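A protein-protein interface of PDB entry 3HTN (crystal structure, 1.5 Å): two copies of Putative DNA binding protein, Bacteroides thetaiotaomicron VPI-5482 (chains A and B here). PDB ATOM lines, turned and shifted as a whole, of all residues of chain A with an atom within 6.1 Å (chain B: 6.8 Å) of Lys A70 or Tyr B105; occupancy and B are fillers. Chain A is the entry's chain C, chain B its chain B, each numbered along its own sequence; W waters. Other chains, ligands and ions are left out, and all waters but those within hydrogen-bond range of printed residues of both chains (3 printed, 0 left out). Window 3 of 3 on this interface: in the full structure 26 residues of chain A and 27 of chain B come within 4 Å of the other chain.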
ATOM      1  N   LEU A  55     -17.226   1.093  10.824  1.00  0.00           N
ATOM      2  CA  LEU A  55     -18.082   2.053  11.508  1.00  0.00           C
ATOM      3  C   LEU A  55     -17.359   2.583  12.714  1.00  0.00           C
ATOM      4  O   LEU A  55     -16.800   1.793  13.465  1.00  0.00           O
ATOM      5  CB  LEU A  55     -19.335   1.363  12.050  1.00  0.00           C
ATOM      6  CG  LEU A  55     -20.333   2.172  12.867  1.00  0.00           C
ATOM      7  CD1 LEU A  55     -20.960   3.239  12.018  1.00  0.00           C
ATOM      8  CD2 LEU A  55     -21.385   1.225  13.496  1.00  0.00           C
ATOM      9  N   THR A  56     -17.452   3.888  12.928  1.00  0.00           N
ATOM     10  CA  THR A  56     -16.937   4.486  14.145  1.00  0.00           C
ATOM     11  C   THR A  56     -18.040   5.273  14.830  1.00  0.00           C
ATOM     12  O   THR A  56     -18.618   6.150  14.227  1.00  0.00           O
ATOM     13  CB  THR A  56     -15.739   5.389  13.901  1.00  0.00           C
ATOM     14  OG1 THR A  56     -14.704   4.639  13.244  1.00  0.00           O
ATOM     15  CG2 THR A  56     -15.178   5.911  15.216  1.00  0.00           C
ATOM     16  N   LEU A  57     -18.335   4.921  16.086  1.00  0.00           N
ATOM     17  CA  LEU A  57     -19.321   5.582  16.881  1.00  0.00           C
ATOM     18  C   LEU A  57     -18.654   6.274  18.057  1.00  0.00           C
ATOM     19  O   LEU A  57     -17.655   5.780  18.536  1.00  0.00           O
ATOM     20  CB  LEU A  57     -20.316   4.551  17.451  1.00  0.00           C
ATOM     21  CG  LEU A  57     -21.129   3.739  16.439  1.00  0.00           C
ATOM     22  CD1 LEU A  57     -21.993   2.725  17.158  1.00  0.00           C
ATOM     23  CD2 LEU A  57     -21.979   4.658  15.568  1.00  0.00           C
ATOM     24  N   ARG A  58     -19.237   7.373  18.516  1.00  0.00           N
ATOM     25  CA  ARG A  58     -18.736   8.069  19.681  1.00  0.00           C
ATOM     26  C   ARG A  58     -19.729   7.996  20.813  1.00  0.00           C
ATOM     27  O   ARG A  58     -20.902   8.251  20.601  1.00  0.00           O
ATOM     28  CB  ARG A  58     -18.445   9.529  19.357  1.00  0.00           C
ATOM     29  CG  ARG A  58     -18.030  10.367  20.580  1.00  0.00           C
ATOM     30  CD  ARG A  58     -17.530  11.716  20.194  1.00  0.00           C
ATOM     31  NE  ARG A  58     -16.225  11.592  19.598  1.00  0.00           N
ATOM     32  CZ  ARG A  58     -15.554  12.545  18.978  1.00  0.00           C
ATOM     33  NH1 ARG A  58     -16.064  13.739  18.830  1.00  0.00           N
ATOM     34  NH2 ARG A  58     -14.377  12.253  18.486  1.00  0.00           N
ATOM     35  N   PHE A  59     -19.244   7.682  22.014  1.00  0.00           N
ATOM     36  CA  PHE A  59     -20.071   7.679  23.208  1.00  0.00           C
ATOM     37  C   PHE A  59     -19.485   8.712  24.166  1.00  0.00           C
ATOM     38  O   PHE A  59     -18.386   8.559  24.689  1.00  0.00           O
ATOM     39  CB  PHE A  59     -20.172   6.301  23.877  1.00  0.00           C
ATOM     40  CG  PHE A  59     -21.232   6.269  24.917  1.00  0.00           C
ATOM     41  CD1 PHE A  59     -22.545   6.058  24.541  1.00  0.00           C
ATOM     42  CD2 PHE A  59     -20.939   6.546  26.236  1.00  0.00           C
ATOM     43  CE1 PHE A  59     -23.551   6.087  25.507  1.00  0.00           C
ATOM     44  CE2 PHE A  59     -21.942   6.573  27.200  1.00  0.00           C
ATOM     45  CZ  PHE A  59     -23.229   6.361  26.816  1.00  0.00           C
ATOM     46  N   ASP A  68     -15.614   8.199  24.032  1.00  0.00           N
ATOM     47  CA  ASP A  68     -15.087   6.896  23.601  1.00  0.00           C
ATOM     48  C   ASP A  68     -15.450   6.740  22.139  1.00  0.00           C
ATOM     49  O   ASP A  68     -16.627   6.806  21.799  1.00  0.00           O
ATOM     50  CB  ASP A  68     -15.766   5.797  24.456  1.00  0.00           C
ATOM     51  CG  ASP A  68     -15.113   4.468  24.383  1.00  0.00           C
ATOM     52  OD1 ASP A  68     -14.032   4.347  23.802  1.00  0.00           O
ATOM     53  OD2 ASP A  68     -15.627   3.509  25.032  1.00  0.00           O
ATOM     54  N   ASP A  69     -14.467   6.503  21.275  1.00  0.00           N
ATOM     55  CA  ASP A  69     -14.704   6.333  19.840  1.00  0.00           C
ATOM     56  C   ASP A  69     -14.413   4.880  19.523  1.00  0.00           C
ATOM     57  O   ASP A  69     -13.252   4.451  19.570  1.00  0.00           O
ATOM     58  CB  ASP A  69     -13.804   7.237  19.008  1.00  0.00           C
ATOM     59  CG  ASP A  69     -14.116   8.709  19.169  1.00  0.00           C
ATOM     60  OD1 ASP A  69     -15.137   9.045  19.789  1.00  0.00           O
ATOM     61  OD2 ASP A  69     -13.339   9.533  18.628  1.00  0.00           O
ATOM     62  N   LYS A  70     -15.449   4.111  19.182  1.00  0.00           N
ATOM     63  CA  LYS A  70     -15.260   2.699  18.893  1.00  0.00           C
ATOM     64  C   LYS A  70     -15.433   2.443  17.404  1.00  0.00           C
ATOM     65  O   LYS A  70     -16.435   2.828  16.813  1.00  0.00           O
ATOM     66  CB  LYS A  70     -16.235   1.834  19.691  1.00  0.00           C
ATOM     67  CG  LYS A  70     -15.941   0.342  19.526  1.00  0.00           C
ATOM     68  CD  LYS A  70     -16.602  -0.501  20.592  1.00  0.00           C
ATOM     69  CE  LYS A  70     -16.186  -1.922  20.402  1.00  0.00           C
ATOM     70  NZ  LYS A  70     -16.785  -2.879  21.456  1.00  0.00           N
ATOM     71  N   THR A  71     -14.456   1.735  16.841  1.00  0.00           N
ATOM     72  CA  THR A  71     -14.405   1.336  15.438  1.00  0.00           C
ATOM     73  C   THR A  71     -14.621  -0.164  15.301  1.00  0.00           C
ATOM     74  O   THR A  71     -13.900  -0.973  15.889  1.00  0.00           O
ATOM     75  CB  THR A  71     -13.101   1.753  14.790  1.00  0.00           C
ATOM     76  OG1 THR A  71     -12.990   3.178  14.847  1.00  0.00           O
ATOM     77  CG2 THR A  71     -13.047   1.293  13.318  1.00  0.00           C
ATOM     78  N   PHE A  72     -15.660  -0.505  14.539  1.00  0.00           N
ATOM     79  CA  PHE A  72     -16.047  -1.857  14.204  1.00  0.00           C
ATOM     80  C   PHE A  72     -15.560  -2.132  12.776  1.00  0.00           C
ATOM     81  O   PHE A  72     -15.740  -1.282  11.912  1.00  0.00           O
ATOM     82  CB  PHE A  72     -17.565  -1.989  14.302  1.00  0.00           C
ATOM     83  CG  PHE A  72     -18.119  -1.711  15.671  1.00  0.00           C
ATOM     84  CD1 PHE A  72     -18.477  -0.448  16.035  1.00  0.00           C
ATOM     85  CD2 PHE A  72     -18.271  -2.739  16.581  1.00  0.00           C
ATOM     86  CE1 PHE A  72     -19.000  -0.196  17.292  1.00  0.00           C
ATOM     87  CE2 PHE A  72     -18.789  -2.495  17.849  1.00  0.00           C
ATOM     88  CZ  PHE A  72     -19.132  -1.208  18.196  1.00  0.00           C
ATOM     89  N   ALA A 107     -28.183  -5.322  16.858  1.00  0.00           N
ATOM     90  CA  ALA A 107     -28.065  -3.921  16.502  1.00  0.00           C
ATOM     91  C   ALA A 107     -27.074  -3.146  17.372  1.00  0.00           C
ATOM     92  O   ALA A 107     -27.036  -3.352  18.601  1.00  0.00           O
ATOM     93  CB  ALA A 107     -29.439  -3.245  16.511  1.00  0.00           C
ATOM     94  N   LEU A 108     -26.346  -2.224  16.735  1.00  0.00           N
ATOM     95  CA  LEU A 108     -25.501  -1.267  17.394  1.00  0.00           C
ATOM     96  C   LEU A 108     -26.069   0.104  17.062  1.00  0.00           C
ATOM     97  O   LEU A 108     -26.665   0.280  15.986  1.00  0.00           O
ATOM     98  CB  LEU A 108     -24.079  -1.349  16.878  1.00  0.00           C
ATOM     99  CG  LEU A 108     -23.357  -2.695  17.005  1.00  0.00           C
ATOM    100  CD1 LEU A 108     -22.058  -2.610  16.217  1.00  0.00           C
ATOM    101  CD2 LEU A 108     -23.108  -3.050  18.456  1.00  0.00           C
ATOM    102  N   ALA A 109     -25.880   1.075  17.949  1.00  0.00           N
ATOM    103  CA  ALA A 109     -26.469   2.388  17.735  1.00  0.00           C
ATOM    104  C   ALA A 109     -25.691   3.460  18.444  1.00  0.00           C
ATOM    105  O   ALA A 109     -25.139   3.217  19.505  1.00  0.00           O
ATOM    106  CB  ALA A 109     -27.931   2.412  18.216  1.00  0.00           C
ATOM    107  N   GLY A 110     -25.664   4.653  17.842  1.00  0.00           N
ATOM    108  CA  GLY A 110     -25.056   5.780  18.487  1.00  0.00           C
ATOM    109  C   GLY A 110     -24.784   6.957  17.583  1.00  0.00           C
ATOM    110  O   GLY A 110     -25.321   7.057  16.493  1.00  0.00           O
ATOM    111  N   VAL B 100     -32.202   3.325  20.896  1.00  0.00           N
ATOM    112  CA  VAL B 100     -31.132   3.966  21.614  1.00  0.00           C
ATOM    113  C   VAL B 100     -29.873   3.095  21.614  1.00  0.00           C
ATOM    114  O   VAL B 100     -29.964   1.860  21.471  1.00  0.00           O
ATOM    115  CB  VAL B 100     -31.506   4.288  23.084  1.00  0.00           C
ATOM    116  CG1 VAL B 100     -32.764   5.216  23.171  1.00  0.00           C
ATOM    117  CG2 VAL B 100     -31.711   3.037  23.897  1.00  0.00           C
ATOM    118  N   GLY B 101     -28.721   3.744  21.802  1.00  0.00           N
ATOM    119  CA  GLY B 101     -27.444   3.071  22.004  1.00  0.00           C
ATOM    120  C   GLY B 101     -26.952   3.289  23.420  1.00  0.00           C
ATOM    121  O   GLY B 101     -27.076   4.369  23.984  1.00  0.00           O
ATOM    122  N   ARG B 102     -26.415   2.223  23.999  1.00  0.00           N
ATOM    123  CA  ARG B 102     -25.877   2.222  25.345  1.00  0.00           C
ATOM    124  C   ARG B 102     -24.387   2.515  25.296  1.00  0.00           C
ATOM    125  O   ARG B 102     -23.796   2.666  24.212  1.00  0.00           O
ATOM    126  CB  ARG B 102     -26.145   0.856  25.996  1.00  0.00           C
ATOM    127  CG  ARG B 102     -27.614   0.433  25.981  1.00  0.00           C
ATOM    128  CD  ARG B 102     -27.825  -0.931  26.603  1.00  0.00           C
ATOM    129  NE  ARG B 102     -27.995  -0.819  28.029  1.00  0.00           N
ATOM    130  CZ  ARG B 102     -28.445  -1.808  28.780  1.00  0.00           C
ATOM    131  NH1 ARG B 102     -28.712  -3.004  28.256  1.00  0.00           N
ATOM    132  NH2 ARG B 102     -28.629  -1.613  30.088  1.00  0.00           N
ATOM    133  N   SER B 103     -23.739   2.590  26.468  1.00  0.00           N
ATOM    134  CA  SER B 103     -22.330   2.876  26.524  1.00  0.00           C
ATOM    135  C   SER B 103     -21.466   1.784  25.913  1.00  0.00           C
ATOM    136  O   SER B 103     -20.289   2.053  25.631  1.00  0.00           O
ATOM    137  CB  SER B 103     -21.916   3.106  27.960  1.00  0.00           C
ATOM    138  OG  SER B 103     -22.056   1.913  28.710  1.00  0.00           O
ATOM    139  N   ASP B 104     -22.014   0.578  25.730  1.00  0.00           N
ATOM    140  CA  ASP B 104     -21.321  -0.491  24.995  1.00  0.00           C
ATOM    141  C   ASP B 104     -21.752  -0.588  23.537  1.00  0.00           C
ATOM    142  O   ASP B 104     -21.400  -1.533  22.840  1.00  0.00           O
ATOM    143  CB  ASP B 104     -21.500  -1.836  25.694  1.00  0.00           C
ATOM    144  CG  ASP B 104     -22.934  -2.382  25.609  1.00  0.00           C
ATOM    145  OD1 ASP B 104     -23.839  -1.673  25.134  1.00  0.00           O
ATOM    146  OD2 ASP B 104     -23.173  -3.549  26.036  1.00  0.00           O
ATOM    147  N   TYR B 105     -22.479   0.424  23.107  1.00  0.00           N
ATOM    148  CA  TYR B 105     -22.935   0.579  21.727  1.00  0.00           C
ATOM    149  C   TYR B 105     -24.042  -0.376  21.327  1.00  0.00           C
ATOM    150  O   TYR B 105     -24.514  -0.303  20.212  1.00  0.00           O
ATOM    151  CB  TYR B 105     -21.765   0.563  20.706  1.00  0.00           C
ATOM    152  CG  TYR B 105     -20.657   1.549  21.091  1.00  0.00           C
ATOM    153  CD1 TYR B 105     -20.748   2.902  20.736  1.00  0.00           C
ATOM    154  CD2 TYR B 105     -19.593   1.134  21.816  1.00  0.00           C
ATOM    155  CE1 TYR B 105     -19.771   3.776  21.120  1.00  0.00           C
ATOM    156  CE2 TYR B 105     -18.617   2.007  22.186  1.00  0.00           C
ATOM    157  CZ  TYR B 105     -18.708   3.309  21.832  1.00  0.00           C
ATOM    158  OH  TYR B 105     -17.648   4.108  22.252  1.00  0.00           O
ATOM    159  N   SER B 106     -24.455  -1.281  22.209  1.00  0.00           N
ATOM    160  CA  SER B 106     -25.604  -2.114  21.920  1.00  0.00           C
ATOM    161  C   SER B 106     -26.854  -1.273  21.877  1.00  0.00           C
ATOM    162  O   SER B 106     -26.922  -0.213  22.513  1.00  0.00           O
ATOM    163  CB  SER B 106     -25.744  -3.221  22.978  1.00  0.00           C
ATOM    164  OG  SER B 106     -26.100  -2.696  24.248  1.00  0.00           O
ATOM    165  N   ALA B 107     -27.825  -1.715  21.083  1.00  0.00           N
ATOM    166  CA  ALA B 107     -29.058  -0.982  20.884  1.00  0.00           C
ATOM    167  C   ALA B 107     -30.211  -1.605  21.636  1.00  0.00           C
ATOM    168  O   ALA B 107     -30.333  -2.852  21.701  1.00  0.00           O
ATOM    169  CB  ALA B 107     -29.387  -0.885  19.367  1.00  0.00           C
HETATM  170  O   HOH W   1     -18.317   3.917  26.025  1.00  0.00           O
HETATM  171  O   HOH W   2     -24.062   4.436  21.780  1.00  0.00           O
HETATM  172  O   HOH W   3     -19.683  -2.872  21.187  1.00  0.00           O
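The backbone carbonyl oxygen (O) of Asp A68 lies within hydrogen-bond range of the side-chain hydroxyl (OH) of Tyr B105, at 2.9 Å.
O of Tyr B105 lies within hydrogen-bond range of N of Ala A109 (3.0 Å).
The backbone carbonyl oxygen of Ala A107 lies within hydrogen-bond range of the backbone NH of Ala B107, 3.1 Å away.
The backbone NH of Lys A70 lies within hydrogen-bond range of the backbone carbonyl oxygen of Leu A57, 2.8 Å away.
OG of Ser B106 lies within hydrogen-bond range of OD1 of Asp B104.
O of Asp A68 lies within hydrogen-bond range of N of Phe A59, 2.8 Å away.
CB of Leu A57 touches CD1 of Tyr B105, at 3.7 Å.
Arg B102 touches Phe A59.
Phe A59 touches Ser B103 (CE2 to CB, 3.5 Å).
CB of Phe A59 touches OH of Tyr B105 (3.7 Å).
CB of Lys A70 touches CE2 of Tyr B105, at 3.5 Å.
O of Ala A107 touches CA of Ser B106, at 3.8 Å.
Leu A108 touches Tyr B105 (CA to O, 3.1 Å).
CB of Ala A109 touches O of Val B100, 3.9 Å away.
Ala A109 touches Gly B101.
CB of Ala B107 touches CB of Ala A109 (3.8 Å).
Of chain B, only Tyr B105 (3.5 Å) comes within 4 Å of Lys A70.
Tyr B105 touches just these residues of chain A: Leu A57 (3.7 Å), Phe A59 (3.7 Å), Asp A68 (2.9 Å), Lys A70 (3.5 Å), Leu A108 (3.1 Å) and Ala A109 (3.0 Å).
Of the printed residues of chain A, Ala B107 touches Ala A107 (3.1 Å) and Ala A109 (3.8 Å).
Of the printed residues of chain B, Ala A109 touches Val B100 (3.9 Å), Gly B101 (3.4 Å), Tyr B105 (3.0 Å) and Ala B107 (3.8 Å).
Printed residues of chain B within 4 Å of Asp A68: Tyr B105.
Printed residues of chain B within 4 Å of Ala A107: Ser B106 (3.8 Å) and Ala B107 (3.1 Å).
Printed residues of chain A within 4 Å of Arg B102: Phe A59 (3.6 Å).
Of the 14 printed residues of chain A, 7 touch a printed residue of chain B.
Hydrophobic or aromatic side chains of chain A that line the printed part of chain B: Leu A57, Phe A59, Ala A107, Leu A108 and Ala A109.
Printed residues of chain B that touch a printed residue of chain A: Val B100, Gly B101, Arg B102, Ser B103, Tyr B105, Ser B106 and Ala B107.
Hydrophobic or aromatic side chains of chain B within 4 Å of the printed part of chain A: Tyr B105 and Ala B107.
Ala B107 touches its own counterpart, Ala A107.
Water W3 lies within hydrogen-bond range of the backbone carbonyl oxygen of Asp B104 and the side-chain amino group of Lys A70.
Water W1 lies within hydrogen-bond range of the backbone carbonyl oxygen of Ser B103 and the side-chain carboxylate of Asp A68.
Water W2 lies within hydrogen-bond range of O of Ala A109 and O of Arg B102.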
